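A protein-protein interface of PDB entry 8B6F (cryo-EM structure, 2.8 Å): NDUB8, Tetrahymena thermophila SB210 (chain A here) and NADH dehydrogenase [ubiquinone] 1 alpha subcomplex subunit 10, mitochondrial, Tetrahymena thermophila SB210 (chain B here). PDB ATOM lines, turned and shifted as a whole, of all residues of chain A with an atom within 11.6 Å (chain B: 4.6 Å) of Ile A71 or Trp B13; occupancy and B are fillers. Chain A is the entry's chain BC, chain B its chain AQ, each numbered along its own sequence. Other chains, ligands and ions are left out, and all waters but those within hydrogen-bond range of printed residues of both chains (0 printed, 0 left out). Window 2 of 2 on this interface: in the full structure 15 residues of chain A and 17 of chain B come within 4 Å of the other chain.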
ATOM      1  N   TYR A  64      19.343 -12.645  23.214  1.00  0.00           N
ATOM      2  CA  TYR A  64      18.724 -13.475  22.195  1.00  0.00           C
ATOM      3  C   TYR A  64      19.728 -13.770  21.086  1.00  0.00           C
ATOM      4  O   TYR A  64      20.595 -12.953  20.768  1.00  0.00           O
ATOM      5  CB  TYR A  64      17.490 -12.779  21.623  1.00  0.00           C
ATOM      6  CG  TYR A  64      16.501 -13.704  20.952  1.00  0.00           C
ATOM      7  CD1 TYR A  64      15.662 -14.517  21.701  1.00  0.00           C
ATOM      8  CD2 TYR A  64      16.388 -13.746  19.571  1.00  0.00           C
ATOM      9  CE1 TYR A  64      14.751 -15.357  21.093  1.00  0.00           C
ATOM     10  CE2 TYR A  64      15.481 -14.581  18.953  1.00  0.00           C
ATOM     11  CZ  TYR A  64      14.666 -15.384  19.719  1.00  0.00           C
ATOM     12  OH  TYR A  64      13.760 -16.217  19.108  1.00  0.00           O
ATOM     13  N   ILE A  66      19.529 -13.733  18.047  1.00  0.00           N
ATOM     14  CA  ILE A  66      19.423 -12.847  16.896  1.00  0.00           C
ATOM     15  C   ILE A  66      18.965 -11.479  17.377  1.00  0.00           C
ATOM     16  O   ILE A  66      18.013 -11.375  18.158  1.00  0.00           O
ATOM     17  CB  ILE A  66      18.451 -13.407  15.840  1.00  0.00           C
ATOM     18  CG1 ILE A  66      18.866 -14.829  15.450  1.00  0.00           C
ATOM     19  CG2 ILE A  66      18.425 -12.512  14.616  1.00  0.00           C
ATOM     20  CD1 ILE A  66      17.898 -15.526  14.522  1.00  0.00           C
ATOM     21  N   SER A  67      19.641 -10.433  16.909  1.00  0.00           N
ATOM     22  CA  SER A  67      19.301  -9.055  17.237  1.00  0.00           C
ATOM     23  C   SER A  67      18.540  -8.433  16.074  1.00  0.00           C
ATOM     24  O   SER A  67      18.949  -8.567  14.917  1.00  0.00           O
ATOM     25  CB  SER A  67      20.557  -8.237  17.535  1.00  0.00           C
ATOM     26  OG  SER A  67      21.225  -8.717  18.687  1.00  0.00           O
ATOM     27  N   TYR A  68      17.440  -7.753  16.384  1.00  0.00           N
ATOM     28  CA  TYR A  68      16.598  -7.096  15.386  1.00  0.00           C
ATOM     29  C   TYR A  68      16.624  -5.595  15.661  1.00  0.00           C
ATOM     30  O   TYR A  68      15.775  -5.069  16.384  1.00  0.00           O
ATOM     31  CB  TYR A  68      15.185  -7.649  15.423  1.00  0.00           C
ATOM     32  CG  TYR A  68      15.127  -9.139  15.201  1.00  0.00           C
ATOM     33  CD1 TYR A  68      15.518  -9.695  13.990  1.00  0.00           C
ATOM     34  CD2 TYR A  68      14.683  -9.991  16.201  1.00  0.00           C
ATOM     35  CE1 TYR A  68      15.469 -11.054  13.784  1.00  0.00           C
ATOM     36  CE2 TYR A  68      14.631 -11.352  16.004  1.00  0.00           C
ATOM     37  CZ  TYR A  68      15.027 -11.878  14.792  1.00  0.00           C
ATOM     38  OH  TYR A  68      14.975 -13.233  14.593  1.00  0.00           O
ATOM     39  N   ASN A  69      17.608  -4.909  15.077  1.00  0.00           N
ATOM     40  CA  ASN A  69      17.708  -3.464  15.253  1.00  0.00           C
ATOM     41  C   ASN A  69      16.590  -2.740  14.517  1.00  0.00           C
ATOM     42  O   ASN A  69      16.054  -1.746  15.017  1.00  0.00           O
ATOM     43  CB  ASN A  69      19.072  -2.975  14.767  1.00  0.00           C
ATOM     44  CG  ASN A  69      20.215  -3.560  15.565  1.00  0.00           C
ATOM     45  OD1 ASN A  69      20.149  -3.652  16.789  1.00  0.00           O
ATOM     46  ND2 ASN A  69      21.273  -3.967  14.872  1.00  0.00           N
ATOM     47  N   GLU A  70      16.227  -3.219  13.328  1.00  0.00           N
ATOM     48  CA  GLU A  70      15.163  -2.606  12.534  1.00  0.00           C
ATOM     49  C   GLU A  70      13.800  -3.112  13.010  1.00  0.00           C
ATOM     50  O   GLU A  70      13.016  -3.695  12.265  1.00  0.00           O
ATOM     51  CB  GLU A  70      15.370  -2.893  11.053  1.00  0.00           C
ATOM     52  CG  GLU A  70      16.719  -2.449  10.507  1.00  0.00           C
ATOM     53  CD  GLU A  70      17.829  -3.441  10.797  1.00  0.00           C
ATOM     54  OE1 GLU A  70      17.596  -4.387  11.578  1.00  0.00           O
ATOM     55  OE2 GLU A  70      18.935  -3.279  10.239  1.00  0.00           O
ATOM     56  N   ILE A  71      13.527  -2.869  14.292  1.00  0.00           N
ATOM     57  CA  ILE A  71      12.303  -3.385  14.893  1.00  0.00           C
ATOM     58  C   ILE A  71      11.095  -2.520  14.569  1.00  0.00           C
ATOM     59  O   ILE A  71       9.957  -2.973  14.742  1.00  0.00           O
ATOM     60  CB  ILE A  71      12.478  -3.521  16.416  1.00  0.00           C
ATOM     61  CG1 ILE A  71      11.318  -4.305  17.039  1.00  0.00           C
ATOM     62  CG2 ILE A  71      12.594  -2.156  17.068  1.00  0.00           C
ATOM     63  CD1 ILE A  71      11.137  -5.712  16.495  1.00  0.00           C
ATOM     64  N   HIS A  72      11.301  -1.291  14.089  1.00  0.00           N
ATOM     65  CA  HIS A  72      10.167  -0.474  13.673  1.00  0.00           C
ATOM     66  C   HIS A  72       9.357  -1.179  12.596  1.00  0.00           C
ATOM     67  O   HIS A  72       8.157  -0.924  12.452  1.00  0.00           O
ATOM     68  CB  HIS A  72      10.649   0.895  13.187  1.00  0.00           C
ATOM     69  CG  HIS A  72      11.575   0.831  12.014  1.00  0.00           C
ATOM     70  ND1 HIS A  72      12.911   0.514  12.137  1.00  0.00           N
ATOM     71  CD2 HIS A  72      11.363   1.053  10.696  1.00  0.00           C
ATOM     72  CE1 HIS A  72      13.478   0.537  10.944  1.00  0.00           C
ATOM     73  NE2 HIS A  72      12.561   0.863  10.053  1.00  0.00           N
ATOM     74  N   LEU A  73       9.994  -2.061  11.830  1.00  0.00           N
ATOM     75  CA  LEU A  73       9.280  -2.969  10.944  1.00  0.00           C
ATOM     76  C   LEU A  73       8.781  -4.148  11.769  1.00  0.00           C
ATOM     77  O   LEU A  73       9.577  -4.849  12.401  1.00  0.00           O
ATOM     78  CB  LEU A  73      10.198  -3.444   9.821  1.00  0.00           C
ATOM     79  CG  LEU A  73      10.942  -2.340   9.070  1.00  0.00           C
ATOM     80  CD1 LEU A  73      12.055  -2.933   8.236  1.00  0.00           C
ATOM     81  CD2 LEU A  73       9.987  -1.542   8.201  1.00  0.00           C
ATOM     82  N   VAL A  74       7.466  -4.364  11.772  1.00  0.00           N
ATOM     83  CA  VAL A  74       6.885  -5.363  12.665  1.00  0.00           C
ATOM     84  C   VAL A  74       7.406  -6.754  12.325  1.00  0.00           C
ATOM     85  O   VAL A  74       7.784  -7.529  13.211  1.00  0.00           O
ATOM     86  CB  VAL A  74       5.349  -5.304  12.607  1.00  0.00           C
ATOM     87  CG1 VAL A  74       4.735  -6.317  13.563  1.00  0.00           C
ATOM     88  CG2 VAL A  74       4.858  -3.899  12.931  1.00  0.00           C
ATOM     89  N   ASP A  75       7.439  -7.092  11.038  1.00  0.00           N
ATOM     90  CA  ASP A  75       7.845  -8.421  10.610  1.00  0.00           C
ATOM     91  C   ASP A  75       8.557  -8.321   9.270  1.00  0.00           C
ATOM     92  O   ASP A  75       8.619  -7.257   8.651  1.00  0.00           O
ATOM     93  CB  ASP A  75       6.644  -9.370  10.525  1.00  0.00           C
ATOM     94  CG  ASP A  75       5.526  -8.819   9.665  1.00  0.00           C
ATOM     95  OD1 ASP A  75       5.699  -8.755   8.430  1.00  0.00           O
ATOM     96  OD2 ASP A  75       4.471  -8.451  10.224  1.00  0.00           O
ATOM     97  N   GLN A  76       9.103  -9.456   8.827  1.00  0.00           N
ATOM     98  CA  GLN A  76       9.879  -9.470   7.591  1.00  0.00           C
ATOM     99  C   GLN A  76       9.016  -9.103   6.391  1.00  0.00           C
ATOM    100  O   GLN A  76       9.486  -8.435   5.463  1.00  0.00           O
ATOM    101  CB  GLN A  76      10.533 -10.838   7.384  1.00  0.00           C
ATOM    102  CG  GLN A  76       9.578 -12.025   7.295  1.00  0.00           C
ATOM    103  CD  GLN A  76       9.154 -12.544   8.652  1.00  0.00           C
ATOM    104  OE1 GLN A  76       9.351 -11.884   9.671  1.00  0.00           O
ATOM    105  NE2 GLN A  76       8.574 -13.736   8.673  1.00  0.00           N
ATOM    106  N   TRP A  77       7.754  -9.535   6.385  1.00  0.00           N
ATOM    107  CA  TRP A  77       6.885  -9.245   5.249  1.00  0.00           C
ATOM    108  C   TRP A  77       6.717  -7.744   5.065  1.00  0.00           C
ATOM    109  O   TRP A  77       6.877  -7.220   3.957  1.00  0.00           O
ATOM    110  CB  TRP A  77       5.528  -9.923   5.435  1.00  0.00           C
ATOM    111  CG  TRP A  77       5.630 -11.378   5.749  1.00  0.00           C
ATOM    112  CD1 TRP A  77       5.249 -11.994   6.904  1.00  0.00           C
ATOM    113  CD2 TRP A  77       6.157 -12.404   4.900  1.00  0.00           C
ATOM    114  NE1 TRP A  77       5.501 -13.343   6.823  1.00  0.00           N
ATOM    115  CE2 TRP A  77       6.057 -13.619   5.602  1.00  0.00           C
ATOM    116  CE3 TRP A  77       6.699 -12.410   3.611  1.00  0.00           C
ATOM    117  CZ2 TRP A  77       6.481 -14.828   5.062  1.00  0.00           C
ATOM    118  CZ3 TRP A  77       7.120 -13.613   3.075  1.00  0.00           C
ATOM    119  CH2 TRP A  77       7.007 -14.807   3.799  1.00  0.00           C
ATOM    120  N   LYS A  78       6.392  -7.031   6.143  1.00  0.00           N
ATOM    121  CA  LYS A  78       6.382  -5.575   6.074  1.00  0.00           C
ATOM    122  C   LYS A  78       7.766  -5.036   5.741  1.00  0.00           C
ATOM    123  O   LYS A  78       7.888  -3.987   5.100  1.00  0.00           O
ATOM    124  CB  LYS A  78       5.881  -4.985   7.390  1.00  0.00           C
ATOM    125  CG  LYS A  78       4.464  -5.408   7.746  1.00  0.00           C
ATOM    126  CD  LYS A  78       3.971  -4.719   9.011  1.00  0.00           C
ATOM    127  CE  LYS A  78       3.711  -3.236   8.780  1.00  0.00           C
ATOM    128  NZ  LYS A  78       3.145  -2.575   9.991  1.00  0.00           N
ATOM    129  N   GLY A  79       8.816  -5.731   6.176  1.00  0.00           N
ATOM    130  CA  GLY A  79      10.160  -5.346   5.781  1.00  0.00           C
ATOM    131  C   GLY A  79      10.367  -5.443   4.282  1.00  0.00           C
ATOM    132  O   GLY A  79      10.950  -4.546   3.667  1.00  0.00           O
ATOM    133  N   GLU A  82       8.425  -2.530   2.652  1.00  0.00           N
ATOM    134  CA  GLU A  82       9.138  -1.267   2.795  1.00  0.00           C
ATOM    135  C   GLU A  82      10.381  -1.237   1.915  1.00  0.00           C
ATOM    136  O   GLU A  82      10.685  -0.216   1.291  1.00  0.00           O
ATOM    137  CB  GLU A  82       9.513  -1.046   4.260  1.00  0.00           C
ATOM    138  CG  GLU A  82      10.029   0.352   4.570  1.00  0.00           C
ATOM    139  CD  GLU A  82       8.931   1.399   4.549  1.00  0.00           C
ATOM    140  OE1 GLU A  82       7.764   1.037   4.296  1.00  0.00           O
ATOM    141  OE2 GLU A  82       9.236   2.586   4.790  1.00  0.00           O
ATOM    142  N   PHE B  11      12.244  -8.333  21.646  1.00  0.00           N
ATOM    143  CA  PHE B  11      11.147  -7.422  21.934  1.00  0.00           C
ATOM    144  C   PHE B  11      10.316  -7.178  20.682  1.00  0.00           C
ATOM    145  O   PHE B  11      10.851  -7.057  19.578  1.00  0.00           O
ATOM    146  CB  PHE B  11      11.675  -6.092  22.466  1.00  0.00           C
ATOM    147  CG  PHE B  11      12.159  -6.155  23.880  1.00  0.00           C
ATOM    148  CD1 PHE B  11      11.264  -6.270  24.928  1.00  0.00           C
ATOM    149  CD2 PHE B  11      13.508  -6.070  24.164  1.00  0.00           C
ATOM    150  CE1 PHE B  11      11.709  -6.320  26.229  1.00  0.00           C
ATOM    151  CE2 PHE B  11      13.958  -6.117  25.463  1.00  0.00           C
ATOM    152  CZ  PHE B  11      13.057  -6.240  26.498  1.00  0.00           C
ATOM    153  N   SER B  12       9.002  -7.107  20.856  1.00  0.00           N
ATOM    154  CA  SER B  12       8.132  -6.702  19.766  1.00  0.00           C
ATOM    155  C   SER B  12       8.213  -5.191  19.580  1.00  0.00           C
ATOM    156  O   SER B  12       8.769  -4.467  20.409  1.00  0.00           O
ATOM    157  CB  SER B  12       6.692  -7.136  20.033  1.00  0.00           C
ATOM    158  OG  SER B  12       6.191  -6.548  21.220  1.00  0.00           O
ATOM    159  N   TRP B  13       7.651  -4.707  18.472  1.00  0.00           N
ATOM    160  CA  TRP B  13       7.708  -3.274  18.206  1.00  0.00           C
ATOM    161  C   TRP B  13       6.974  -2.482  19.280  1.00  0.00           C
ATOM    162  O   TRP B  13       7.445  -1.423  19.710  1.00  0.00           O
ATOM    163  CB  TRP B  13       7.125  -2.953  16.833  1.00  0.00           C
ATOM    164  CG  TRP B  13       6.848  -1.492  16.687  1.00  0.00           C
ATOM    165  CD1 TRP B  13       5.658  -0.910  16.371  1.00  0.00           C
ATOM    166  CD2 TRP B  13       7.779  -0.422  16.887  1.00  0.00           C
ATOM    167  NE1 TRP B  13       5.792   0.456  16.351  1.00  0.00           N
ATOM    168  CE2 TRP B  13       7.086   0.780  16.663  1.00  0.00           C
ATOM    169  CE3 TRP B  13       9.134  -0.367  17.227  1.00  0.00           C
ATOM    170  CZ2 TRP B  13       7.700   2.024  16.767  1.00  0.00           C
ATOM    171  CZ3 TRP B  13       9.743   0.870  17.330  1.00  0.00           C
ATOM    172  CH2 TRP B  13       9.028   2.049  17.099  1.00  0.00           C
ATOM    173  N   ALA B  14       5.821  -2.978  19.730  1.00  0.00           N
ATOM    174  CA  ALA B  14       5.084  -2.272  20.770  1.00  0.00           C
ATOM    175  C   ALA B  14       5.897  -2.191  22.054  1.00  0.00           C
ATOM    176  O   ALA B  14       5.937  -1.144  22.708  1.00  0.00           O
ATOM    177  CB  ALA B  14       3.746  -2.964  21.026  1.00  0.00           C
ATOM    178  N   GLU B  15       6.549  -3.290  22.432  1.00  0.00           N
ATOM    179  CA  GLU B  15       7.371  -3.284  23.637  1.00  0.00           C
ATOM    180  C   GLU B  15       8.551  -2.330  23.495  1.00  0.00           C
ATOM    181  O   GLU B  15       8.892  -1.609  24.438  1.00  0.00           O
ATOM    182  CB  GLU B  15       7.855  -4.702  23.935  1.00  0.00           C
ATOM    183  CG  GLU B  15       6.722  -5.692  24.165  1.00  0.00           C
ATOM    184  CD  GLU B  15       7.189  -7.133  24.145  1.00  0.00           C
ATOM    185  OE1 GLU B  15       8.411  -7.361  24.032  1.00  0.00           O
ATOM    186  OE2 GLU B  15       6.335  -8.038  24.237  1.00  0.00           O
ATOM    187  N   VAL B  16       9.188  -2.312  22.322  1.00  0.00           N
ATOM    188  CA  VAL B  16      10.314  -1.408  22.104  1.00  0.00           C
ATOM    189  C   VAL B  16       9.848   0.039  22.158  1.00  0.00           C
ATOM    190  O   VAL B  16      10.523   0.902  22.732  1.00  0.00           O
ATOM    191  CB  VAL B  16      11.017  -1.724  20.770  1.00  0.00           C
ATOM    192  CG1 VAL B  16      12.069  -0.661  20.452  1.00  0.00           C
ATOM    193  CG2 VAL B  16      11.653  -3.099  20.818  1.00  0.00           C
ATOM    194  N   SER B  17       8.691   0.330  21.565  1.00  0.00           N
ATOM    195  CA  SER B  17       8.164   1.688  21.617  1.00  0.00           C
ATOM    196  C   SER B  17       7.864   2.102  23.050  1.00  0.00           C
ATOM    197  O   SER B  17       8.152   3.235  23.451  1.00  0.00           O
ATOM    198  CB  SER B  17       6.905   1.791  20.756  1.00  0.00           C
ATOM    199  OG  SER B  17       6.344   3.090  20.825  1.00  0.00           O
ATOM    200  N   GLU B  98       8.419   7.180  17.250  1.00  0.00           N
ATOM    201  CA  GLU B  98       8.554   6.170  16.207  1.00  0.00           C
ATOM    202  C   GLU B  98       9.181   6.761  14.951  1.00  0.00           C
ATOM    203  O   GLU B  98      10.043   6.138  14.324  1.00  0.00           O
ATOM    204  CB  GLU B  98       7.190   5.555  15.893  1.00  0.00           C
ATOM    205  CG  GLU B  98       7.209   4.536  14.758  1.00  0.00           C
ATOM    206  CD  GLU B  98       7.101   5.166  13.381  1.00  0.00           C
ATOM    207  OE1 GLU B  98       6.807   6.377  13.297  1.00  0.00           O
ATOM    208  OE2 GLU B  98       7.311   4.448  12.382  1.00  0.00           O
ATOM    209  N   PHE B 101      12.760   7.192  15.456  1.00  0.00           N
ATOM    210  CA  PHE B 101      13.479   5.968  15.780  1.00  0.00           C
ATOM    211  C   PHE B 101      14.574   5.718  14.754  1.00  0.00           C
ATOM    212  O   PHE B 101      14.329   5.732  13.546  1.00  0.00           O
ATOM    213  CB  PHE B 101      12.522   4.777  15.821  1.00  0.00           C
ATOM    214  CG  PHE B 101      13.210   3.459  16.027  1.00  0.00           C
ATOM    215  CD1 PHE B 101      13.551   3.032  17.298  1.00  0.00           C
ATOM    216  CD2 PHE B 101      13.522   2.649  14.949  1.00  0.00           C
ATOM    217  CE1 PHE B 101      14.187   1.823  17.490  1.00  0.00           C
ATOM    218  CE2 PHE B 101      14.158   1.441  15.135  1.00  0.00           C
ATOM    219  CZ  PHE B 101      14.490   1.027  16.407  1.00  0.00           C
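Among the printed residues, pairs that only touch across the chains: Asn A69 with Phe B101, Ile A71 with Phe B11, Ile A71 with Trp B13, Ile A71 with Val B16, Ile A71 with Phe B101, His A72 with Trp B13 and His A72 with Phe B101.
Of chain B, only Phe B11 (3.4 Å), Trp B13 (3.5 Å), Val B16 (3.7 Å) and Phe B101 (3.8 Å) come within 4 Å of Ile A71.
Of chain A, only Ile A71 and His A72 come within 4 Å of Trp B13.
No residue of chain A comes within 4 Å of Ser B12.
No residue of chain A comes within 4 Å of Ala B14.
No residue of chain A comes within 4 Å of Glu B15.
No residue of chain A comes within 4 Å of Ser B17.
Phe B101 touches three residues of chain A.
Printed residues of chain B within 4 Å of His A72: Trp B13 (3.7 Å) and Phe B101 (3.4 Å).
Of the printed residues of chain A, Phe B11 touches Ile A71 (3.4 Å).
Lys A78 touches none of the printed residues of chain B.
The nearest printed residue of chain B that does not touch His A72 is Glu B98 (4.9 Å).
Of the 9 printed residues of chain B, 4 touch a printed residue of chain A.
Hydrophobic or aromatic side chains of chain B within 4 Å of the printed part of chain A: Trp B13, Val B16 and Phe B101.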
